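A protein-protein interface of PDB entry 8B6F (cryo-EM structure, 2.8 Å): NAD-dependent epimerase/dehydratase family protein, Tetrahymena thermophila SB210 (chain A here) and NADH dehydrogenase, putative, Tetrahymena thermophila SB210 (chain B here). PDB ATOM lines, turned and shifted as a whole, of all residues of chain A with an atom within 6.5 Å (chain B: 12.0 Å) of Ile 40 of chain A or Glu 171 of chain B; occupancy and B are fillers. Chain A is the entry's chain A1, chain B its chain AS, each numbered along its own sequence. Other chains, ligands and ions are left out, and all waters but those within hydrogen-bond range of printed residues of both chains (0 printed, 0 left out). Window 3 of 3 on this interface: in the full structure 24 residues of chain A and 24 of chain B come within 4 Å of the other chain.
The backbone NH of Tyr 32 of chain A is in hydrogen-bond range of the backbone carbonyl oxygen of Ser 41 of chain A (2.7 Å).
O of Ser 39 of chain A is in hydrogen-bond range of NE2 of Gln 94 of chain A, 3.5 Å away.
The side-chain amide nitrogen (ND2) of Asn 117 of chain A is in hydrogen-bond range of the backbone carbonyl oxygen (O) of Gly 42 of chain A, at 3.5 Å.
NZ of Lys 168 of chain B lies within hydrogen-bond range of O of Phe 172 of chain B, at 2.7 Å.
Among the printed residues, merely in contact across the chains: Tyr 32 of chain A with Lys 165 of chain B (3.96 Å), Tyr 32 of chain A with Gly 166 of chain B (3.5 Å), Tyr 32 of chain A with Asn 167 of chain B (3.8 Å), Tyr 32 of chain A with Lys 168 of chain B (3.96 Å), Ser 39 of chain A with Pro 169 of chain B (3.5 Å), Ile 40 of chain A with Pro 169 of chain B (3.5 Å), Ile 40 of chain A with Glu 171 of chain B (3.6 Å) and Gly 42 of chain A with Glu 171 of chain B (3.5 Å).
Ile 40 of chain A touches two residues of chain B.
Of chain A, only Ile 40 and Gly 42 come within 4 Å of Glu 171 of chain B.
No residue of chain B comes within 4 Å of Ser 41 of chain A.
Gly 42 of chain A touches one residue of chain B.
No residue of chain B comes within 4 Å of Ser 67 of chain A.
Of the printed residues of chain A, Gly 166 of chain B touches Tyr 32 (3.5 Å).
Of the printed residues of chain A, Asn 167 of chain B touches Tyr 32.
Of the printed residues of chain A, Lys 168 of chain B touches Tyr 32 (3.96 Å).
Ile 43 of chain A touches none of the printed residues of chain B.
The nearest residue of chain A that does not touch Glu 171 of chain B is Lys 30 of chain A (4.5 Å).
The nearest printed residue of chain A that does not touch Lys 168 of chain B is Ser 39 of chain A (6.3 Å).
Hydrophobic or aromatic side chains of chain A that line the printed part of chain B: Tyr 32 and Ile 40.
Hydrophobic or aromatic side chains of chain B within 4 Å of the printed part of chain A: Pro 169.
Among the printed residues, 8 pairs touch across the chains.
Among the printed residues, no Asp or Glu carboxylate lies within 4 Å of a Lys or Arg side-chain nitrogen of the other chain.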
ATOM      1  N   LYS A  30     -15.735  27.295  20.776  1.00  0.00           N
ATOM      2  CA  LYS A  30     -15.641  26.142  19.886  1.00  0.00           C
ATOM      3  C   LYS A  30     -14.200  26.018  19.408  1.00  0.00           C
ATOM      4  O   LYS A  30     -13.732  26.835  18.610  1.00  0.00           O
ATOM      5  CB  LYS A  30     -16.594  26.297  18.704  1.00  0.00           C
ATOM      6  CG  LYS A  30     -17.706  25.264  18.646  1.00  0.00           C
ATOM      7  CD  LYS A  30     -18.618  25.517  17.450  1.00  0.00           C
ATOM      8  CE  LYS A  30     -19.732  24.487  17.359  1.00  0.00           C
ATOM      9  NZ  LYS A  30     -19.211  23.111  17.141  1.00  0.00           N
ATOM     10  N   PHE A  31     -13.495  24.998  19.892  1.00  0.00           N
ATOM     11  CA  PHE A  31     -12.124  24.755  19.475  1.00  0.00           C
ATOM     12  C   PHE A  31     -11.883  23.256  19.374  1.00  0.00           C
ATOM     13  O   PHE A  31     -12.541  22.457  20.044  1.00  0.00           O
ATOM     14  CB  PHE A  31     -11.112  25.397  20.437  1.00  0.00           C
ATOM     15  CG  PHE A  31     -11.011  24.712  21.769  1.00  0.00           C
ATOM     16  CD1 PHE A  31     -11.892  25.020  22.790  1.00  0.00           C
ATOM     17  CD2 PHE A  31     -10.016  23.780  22.007  1.00  0.00           C
ATOM     18  CE1 PHE A  31     -11.792  24.398  24.020  1.00  0.00           C
ATOM     19  CE2 PHE A  31      -9.911  23.156  23.233  1.00  0.00           C
ATOM     20  CZ  PHE A  31     -10.800  23.466  24.242  1.00  0.00           C
ATOM     21  N   TYR A  32     -10.934  22.889  18.518  1.00  0.00           N
ATOM     22  CA  TYR A  32     -10.580  21.500  18.256  1.00  0.00           C
ATOM     23  C   TYR A  32      -9.253  21.200  18.938  1.00  0.00           C
ATOM     24  O   TYR A  32      -8.237  21.831  18.630  1.00  0.00           O
ATOM     25  CB  TYR A  32     -10.490  21.248  16.751  1.00  0.00           C
ATOM     26  CG  TYR A  32     -10.039  19.857  16.379  1.00  0.00           C
ATOM     27  CD1 TYR A  32     -10.840  18.754  16.629  1.00  0.00           C
ATOM     28  CD2 TYR A  32      -8.817  19.652  15.752  1.00  0.00           C
ATOM     29  CE1 TYR A  32     -10.432  17.481  16.281  1.00  0.00           C
ATOM     30  CE2 TYR A  32      -8.400  18.386  15.399  1.00  0.00           C
ATOM     31  CZ  TYR A  32      -9.212  17.305  15.665  1.00  0.00           C
ATOM     32  OH  TYR A  32      -8.797  16.041  15.314  1.00  0.00           O
ATOM     33  N   GLY A  35      -5.606  18.282  17.387  1.00  0.00           N
ATOM     34  CA  GLY A  35      -4.530  18.564  16.456  1.00  0.00           C
ATOM     35  C   GLY A  35      -3.226  18.933  17.132  1.00  0.00           C
ATOM     36  O   GLY A  35      -3.204  19.264  18.321  1.00  0.00           O
ATOM     37  N   ASN A  36      -2.131  18.871  16.381  1.00  0.00           N
ATOM     38  CA  ASN A  36      -0.812  19.211  16.890  1.00  0.00           C
ATOM     39  C   ASN A  36      -0.528  20.690  16.630  1.00  0.00           C
ATOM     40  O   ASN A  36      -1.419  21.464  16.271  1.00  0.00           O
ATOM     41  CB  ASN A  36       0.239  18.296  16.266  1.00  0.00           C
ATOM     42  CG  ASN A  36       0.163  16.878  16.797  1.00  0.00           C
ATOM     43  OD1 ASN A  36      -0.088  16.659  17.981  1.00  0.00           O
ATOM     44  ND2 ASN A  36       0.379  15.907  15.919  1.00  0.00           N
ATOM     45  N   ARG A  37       0.730  21.099  16.813  1.00  0.00           N
ATOM     46  CA  ARG A  37       1.073  22.517  16.753  1.00  0.00           C
ATOM     47  C   ARG A  37       0.668  23.152  15.430  1.00  0.00           C
ATOM     48  O   ARG A  37       0.322  24.339  15.396  1.00  0.00           O
ATOM     49  CB  ARG A  37       2.573  22.702  16.983  1.00  0.00           C
ATOM     50  CG  ARG A  37       3.049  22.208  18.335  1.00  0.00           C
ATOM     51  CD  ARG A  37       3.898  20.963  18.206  1.00  0.00           C
ATOM     52  NE  ARG A  37       4.371  20.492  19.502  1.00  0.00           N
ATOM     53  CZ  ARG A  37       5.388  21.023  20.168  1.00  0.00           C
ATOM     54  NH1 ARG A  37       6.048  22.070  19.703  1.00  0.00           N
ATOM     55  NH2 ARG A  37       5.752  20.489  21.330  1.00  0.00           N
ATOM     56  N   GLN A  38       0.711  22.397  14.339  1.00  0.00           N
ATOM     57  CA  GLN A  38       0.418  22.937  13.019  1.00  0.00           C
ATOM     58  C   GLN A  38      -1.069  22.936  12.687  1.00  0.00           C
ATOM     59  O   GLN A  38      -1.443  23.370  11.593  1.00  0.00           O
ATOM     60  CB  GLN A  38       1.182  22.151  11.949  1.00  0.00           C
ATOM     61  CG  GLN A  38       2.692  22.206  12.111  1.00  0.00           C
ATOM     62  CD  GLN A  38       3.232  23.622  12.091  1.00  0.00           C
ATOM     63  OE1 GLN A  38       2.601  24.532  11.553  1.00  0.00           O
ATOM     64  NE2 GLN A  38       4.402  23.818  12.686  1.00  0.00           N
ATOM     65  N   SER A  39      -1.919  22.454  13.588  1.00  0.00           N
ATOM     66  CA  SER A  39      -3.355  22.482  13.369  1.00  0.00           C
ATOM     67  C   SER A  39      -3.912  23.859  13.728  1.00  0.00           C
ATOM     68  O   SER A  39      -3.189  24.757  14.166  1.00  0.00           O
ATOM     69  CB  SER A  39      -4.034  21.383  14.182  1.00  0.00           C
ATOM     70  OG  SER A  39      -5.431  21.367  13.952  1.00  0.00           O
ATOM     71  N   ILE A  40      -5.216  24.032  13.530  1.00  0.00           N
ATOM     72  CA  ILE A  40      -5.919  25.260  13.883  1.00  0.00           C
ATOM     73  C   ILE A  40      -6.834  24.918  15.052  1.00  0.00           C
ATOM     74  O   ILE A  40      -7.914  24.347  14.868  1.00  0.00           O
ATOM     75  CB  ILE A  40      -6.707  25.838  12.703  1.00  0.00           C
ATOM     76  CG1 ILE A  40      -5.781  26.038  11.500  1.00  0.00           C
ATOM     77  CG2 ILE A  40      -7.362  27.155  13.106  1.00  0.00           C
ATOM     78  CD1 ILE A  40      -6.477  26.557  10.258  1.00  0.00           C
ATOM     79  N   SER A  41      -6.404  25.269  16.264  1.00  0.00           N
ATOM     80  CA  SER A  41      -7.199  24.959  17.447  1.00  0.00           C
ATOM     81  C   SER A  41      -8.529  25.700  17.432  1.00  0.00           C
ATOM     82  O   SER A  41      -9.571  25.127  17.768  1.00  0.00           O
ATOM     83  CB  SER A  41      -6.414  25.316  18.708  1.00  0.00           C
ATOM     84  OG  SER A  41      -7.183  25.073  19.871  1.00  0.00           O
ATOM     85  N   GLY A  42      -8.514  26.965  17.035  1.00  0.00           N
ATOM     86  CA  GLY A  42      -9.671  27.822  17.150  1.00  0.00           C
ATOM     87  C   GLY A  42      -9.654  28.742  18.348  1.00  0.00           C
ATOM     88  O   GLY A  42     -10.651  29.429  18.593  1.00  0.00           O
ATOM     89  N   ILE A  43      -8.556  28.779  19.097  1.00  0.00           N
ATOM     90  CA  ILE A  43      -8.396  29.667  20.241  1.00  0.00           C
ATOM     91  C   ILE A  43      -7.386  30.740  19.868  1.00  0.00           C
ATOM     92  O   ILE A  43      -6.272  30.430  19.429  1.00  0.00           O
ATOM     93  CB  ILE A  43      -7.940  28.904  21.497  1.00  0.00           C
ATOM     94  CG1 ILE A  43      -8.987  27.860  21.895  1.00  0.00           C
ATOM     95  CG2 ILE A  43      -7.688  29.876  22.644  1.00  0.00           C
ATOM     96  CD1 ILE A  43      -8.571  26.978  23.058  1.00  0.00           C
ATOM     97  N   ARG A  44      -7.775  31.996  20.043  1.00  0.00           N
ATOM     98  CA  ARG A  44      -6.867  33.132  19.960  1.00  0.00           C
ATOM     99  C   ARG A  44      -6.771  33.715  21.361  1.00  0.00           C
ATOM    100  O   ARG A  44      -7.747  34.268  21.877  1.00  0.00           O
ATOM    101  CB  ARG A  44      -7.363  34.159  18.944  1.00  0.00           C
ATOM    102  CG  ARG A  44      -7.154  33.721  17.503  1.00  0.00           C
ATOM    103  CD  ARG A  44      -7.963  34.544  16.518  1.00  0.00           C
ATOM    104  NE  ARG A  44      -9.360  34.125  16.470  1.00  0.00           N
ATOM    105  CZ  ARG A  44     -10.354  34.708  17.127  1.00  0.00           C
ATOM    106  NH1 ARG A  44     -10.152  35.756  17.908  1.00  0.00           N
ATOM    107  NH2 ARG A  44     -11.587  34.227  16.995  1.00  0.00           N
ATOM    108  N   ILE A  65      -1.810  22.777  20.676  1.00  0.00           N
ATOM    109  CA  ILE A  65      -2.968  22.308  19.929  1.00  0.00           C
ATOM    110  C   ILE A  65      -3.254  23.176  18.714  1.00  0.00           C
ATOM    111  O   ILE A  65      -4.255  22.951  18.023  1.00  0.00           O
ATOM    112  CB  ILE A  65      -4.213  22.209  20.834  1.00  0.00           C
ATOM    113  CG1 ILE A  65      -4.526  23.561  21.477  1.00  0.00           C
ATOM    114  CG2 ILE A  65      -3.991  21.145  21.899  1.00  0.00           C
ATOM    115  CD1 ILE A  65      -5.827  23.586  22.245  1.00  0.00           C
ATOM    116  N   GLY A  66      -2.397  24.153  18.427  1.00  0.00           N
ATOM    117  CA  GLY A  66      -2.556  25.014  17.277  1.00  0.00           C
ATOM    118  C   GLY A  66      -3.136  26.381  17.560  1.00  0.00           C
ATOM    119  O   GLY A  66      -3.391  27.131  16.613  1.00  0.00           O
ATOM    120  N   SER A  67      -3.350  26.730  18.824  1.00  0.00           N
ATOM    121  CA  SER A  67      -3.942  28.016  19.153  1.00  0.00           C
ATOM    122  C   SER A  67      -2.951  29.148  18.916  1.00  0.00           C
ATOM    123  O   SER A  67      -1.734  28.975  19.012  1.00  0.00           O
ATOM    124  CB  SER A  67      -4.397  28.032  20.610  1.00  0.00           C
ATOM    125  OG  SER A  67      -5.241  26.928  20.889  1.00  0.00           O
ATOM    126  N   ASP A  68      -3.490  30.324  18.602  1.00  0.00           N
ATOM    127  CA  ASP A  68      -2.676  31.521  18.472  1.00  0.00           C
ATOM    128  C   ASP A  68      -2.477  32.138  19.849  1.00  0.00           C
ATOM    129  O   ASP A  68      -3.437  32.298  20.609  1.00  0.00           O
ATOM    130  CB  ASP A  68      -3.340  32.524  17.530  1.00  0.00           C
ATOM    131  CG  ASP A  68      -3.558  31.958  16.141  1.00  0.00           C
ATOM    132  OD1 ASP A  68      -2.783  31.069  15.730  1.00  0.00           O
ATOM    133  OD2 ASP A  68      -4.503  32.405  15.456  1.00  0.00           O
ATOM    134  N   GLN A  94       2.154  31.665  14.815  1.00  0.00           N
ATOM    135  CA  GLN A  94       1.144  31.431  15.835  1.00  0.00           C
ATOM    136  C   GLN A  94       1.464  32.093  17.165  1.00  0.00           C
ATOM    137  O   GLN A  94       0.539  32.500  17.868  1.00  0.00           O
ATOM    138  CB  GLN A  94       0.960  29.924  16.063  1.00  0.00           C
ATOM    139  CG  GLN A  94       0.423  29.186  14.850  1.00  0.00           C
ATOM    140  CD  GLN A  94       0.394  27.687  15.047  1.00  0.00           C
ATOM    141  OE1 GLN A  94       1.204  27.131  15.785  1.00  0.00           O
ATOM    142  NE2 GLN A  94      -0.549  27.022  14.391  1.00  0.00           N
ATOM    143  N   ASN A 117     -10.028  35.752  21.699  1.00  0.00           N
ATOM    144  CA  ASN A 117     -11.241  35.312  22.374  1.00  0.00           C
ATOM    145  C   ASN A 117     -10.964  34.716  23.748  1.00  0.00           C
ATOM    146  O   ASN A 117     -11.913  34.423  24.482  1.00  0.00           O
ATOM    147  CB  ASN A 117     -11.992  34.293  21.508  1.00  0.00           C
ATOM    148  CG  ASN A 117     -11.107  33.154  21.040  1.00  0.00           C
ATOM    149  OD1 ASN A 117     -10.064  32.880  21.629  1.00  0.00           O
ATOM    150  ND2 ASN A 117     -11.520  32.488  19.970  1.00  0.00           N
ATOM    151  N   LYS B 165     -16.214  14.580  19.576  1.00  0.00           N
ATOM    152  CA  LYS B 165     -14.860  15.123  19.589  1.00  0.00           C
ATOM    153  C   LYS B 165     -14.535  15.829  18.279  1.00  0.00           C
ATOM    154  O   LYS B 165     -13.936  16.910  18.281  1.00  0.00           O
ATOM    155  CB  LYS B 165     -13.852  14.005  19.852  1.00  0.00           C
ATOM    156  CG  LYS B 165     -13.930  13.411  21.251  1.00  0.00           C
ATOM    157  CD  LYS B 165     -13.296  12.027  21.297  1.00  0.00           C
ATOM    158  CE  LYS B 165     -13.420  11.408  22.682  1.00  0.00           C
ATOM    159  NZ  LYS B 165     -12.881  10.018  22.723  1.00  0.00           N
ATOM    160  N   GLY B 166     -14.921  15.238  17.156  1.00  0.00           N
ATOM    161  CA  GLY B 166     -14.577  15.770  15.855  1.00  0.00           C
ATOM    162  C   GLY B 166     -13.257  15.227  15.335  1.00  0.00           C
ATOM    163  O   GLY B 166     -12.439  14.679  16.071  1.00  0.00           O
ATOM    164  N   ASN B 167     -13.057  15.389  14.024  1.00  0.00           N
ATOM    165  CA  ASN B 167     -11.842  14.900  13.383  1.00  0.00           C
ATOM    166  C   ASN B 167     -11.272  15.905  12.386  1.00  0.00           C
ATOM    167  O   ASN B 167     -10.520  15.512  11.486  1.00  0.00           O
ATOM    168  CB  ASN B 167     -12.099  13.569  12.674  1.00  0.00           C
ATOM    169  CG  ASN B 167     -13.077  13.702  11.527  1.00  0.00           C
ATOM    170  OD1 ASN B 167     -13.964  14.553  11.550  1.00  0.00           O
ATOM    171  ND2 ASN B 167     -12.918  12.859  10.515  1.00  0.00           N
ATOM    172  N   LYS B 168     -11.612  17.190  12.517  1.00  0.00           N
ATOM    173  CA  LYS B 168     -11.134  18.207  11.594  1.00  0.00           C
ATOM    174  C   LYS B 168     -11.245  19.559  12.275  1.00  0.00           C
ATOM    175  O   LYS B 168     -12.217  19.779  13.010  1.00  0.00           O
ATOM    176  CB  LYS B 168     -11.954  18.201  10.299  1.00  0.00           C
ATOM    177  CG  LYS B 168     -11.414  19.117   9.213  1.00  0.00           C
ATOM    178  CD  LYS B 168     -12.449  19.374   8.130  1.00  0.00           C
ATOM    179  CE  LYS B 168     -13.462  20.419   8.563  1.00  0.00           C
ATOM    180  NZ  LYS B 168     -12.841  21.762   8.743  1.00  0.00           N
ATOM    181  N   PRO B 169     -10.297  20.474  12.074  1.00  0.00           N
ATOM    182  CA  PRO B 169     -10.465  21.822  12.629  1.00  0.00           C
ATOM    183  C   PRO B 169     -11.737  22.470  12.105  1.00  0.00           C
ATOM    184  O   PRO B 169     -12.065  22.372  10.921  1.00  0.00           O
ATOM    185  CB  PRO B 169      -9.212  22.564  12.149  1.00  0.00           C
ATOM    186  CG  PRO B 169      -8.210  21.500  11.903  1.00  0.00           C
ATOM    187  CD  PRO B 169      -8.985  20.308  11.424  1.00  0.00           C
ATOM    188  N   THR B 170     -12.458  23.137  13.004  1.00  0.00           N
ATOM    189  CA  THR B 170     -13.722  23.767  12.650  1.00  0.00           C
ATOM    190  C   THR B 170     -13.564  25.200  12.160  1.00  0.00           C
ATOM    191  O   THR B 170     -14.505  25.743  11.573  1.00  0.00           O
ATOM    192  CB  THR B 170     -14.674  23.752  13.850  1.00  0.00           C
ATOM    193  OG1 THR B 170     -14.055  24.399  14.969  1.00  0.00           O
ATOM    194  CG2 THR B 170     -15.028  22.324  14.228  1.00  0.00           C
ATOM    195  N   GLU B 171     -12.403  25.823  12.382  1.00  0.00           N
ATOM    196  CA  GLU B 171     -12.205  27.192  11.918  1.00  0.00           C
ATOM    197  C   GLU B 171     -12.244  27.272  10.399  1.00  0.00           C
ATOM    198  O   GLU B 171     -12.825  28.207   9.834  1.00  0.00           O
ATOM    199  CB  GLU B 171     -10.879  27.739  12.443  1.00  0.00           C
ATOM    200  CG  GLU B 171     -10.898  28.112  13.913  1.00  0.00           C
ATOM    201  CD  GLU B 171     -11.804  29.293  14.205  1.00  0.00           C
ATOM    202  OE1 GLU B 171     -12.223  29.974  13.246  1.00  0.00           O
ATOM    203  OE2 GLU B 171     -12.098  29.543  15.392  1.00  0.00           O
ATOM    204  N   PHE B 172     -11.629  26.310   9.720  1.00  0.00           N
ATOM    205  CA  PHE B 172     -11.609  26.291   8.264  1.00  0.00           C
ATOM    206  C   PHE B 172     -12.375  25.084   7.734  1.00  0.00           C
ATOM    207  O   PHE B 172     -11.817  23.996   7.594  1.00  0.00           O
ATOM    208  CB  PHE B 172     -10.170  26.273   7.745  1.00  0.00           C
ATOM    209  CG  PHE B 172     -10.063  26.491   6.266  1.00  0.00           C
ATOM    210  CD1 PHE B 172     -10.180  25.429   5.385  1.00  0.00           C
ATOM    211  CD2 PHE B 172      -9.845  27.759   5.756  1.00  0.00           C
ATOM    212  CE1 PHE B 172     -10.080  25.627   4.025  1.00  0.00           C
ATOM    213  CE2 PHE B 172      -9.744  27.963   4.396  1.00  0.00           C
ATOM    214  CZ  PHE B 172      -9.864  26.896   3.528  1.00  0.00           C
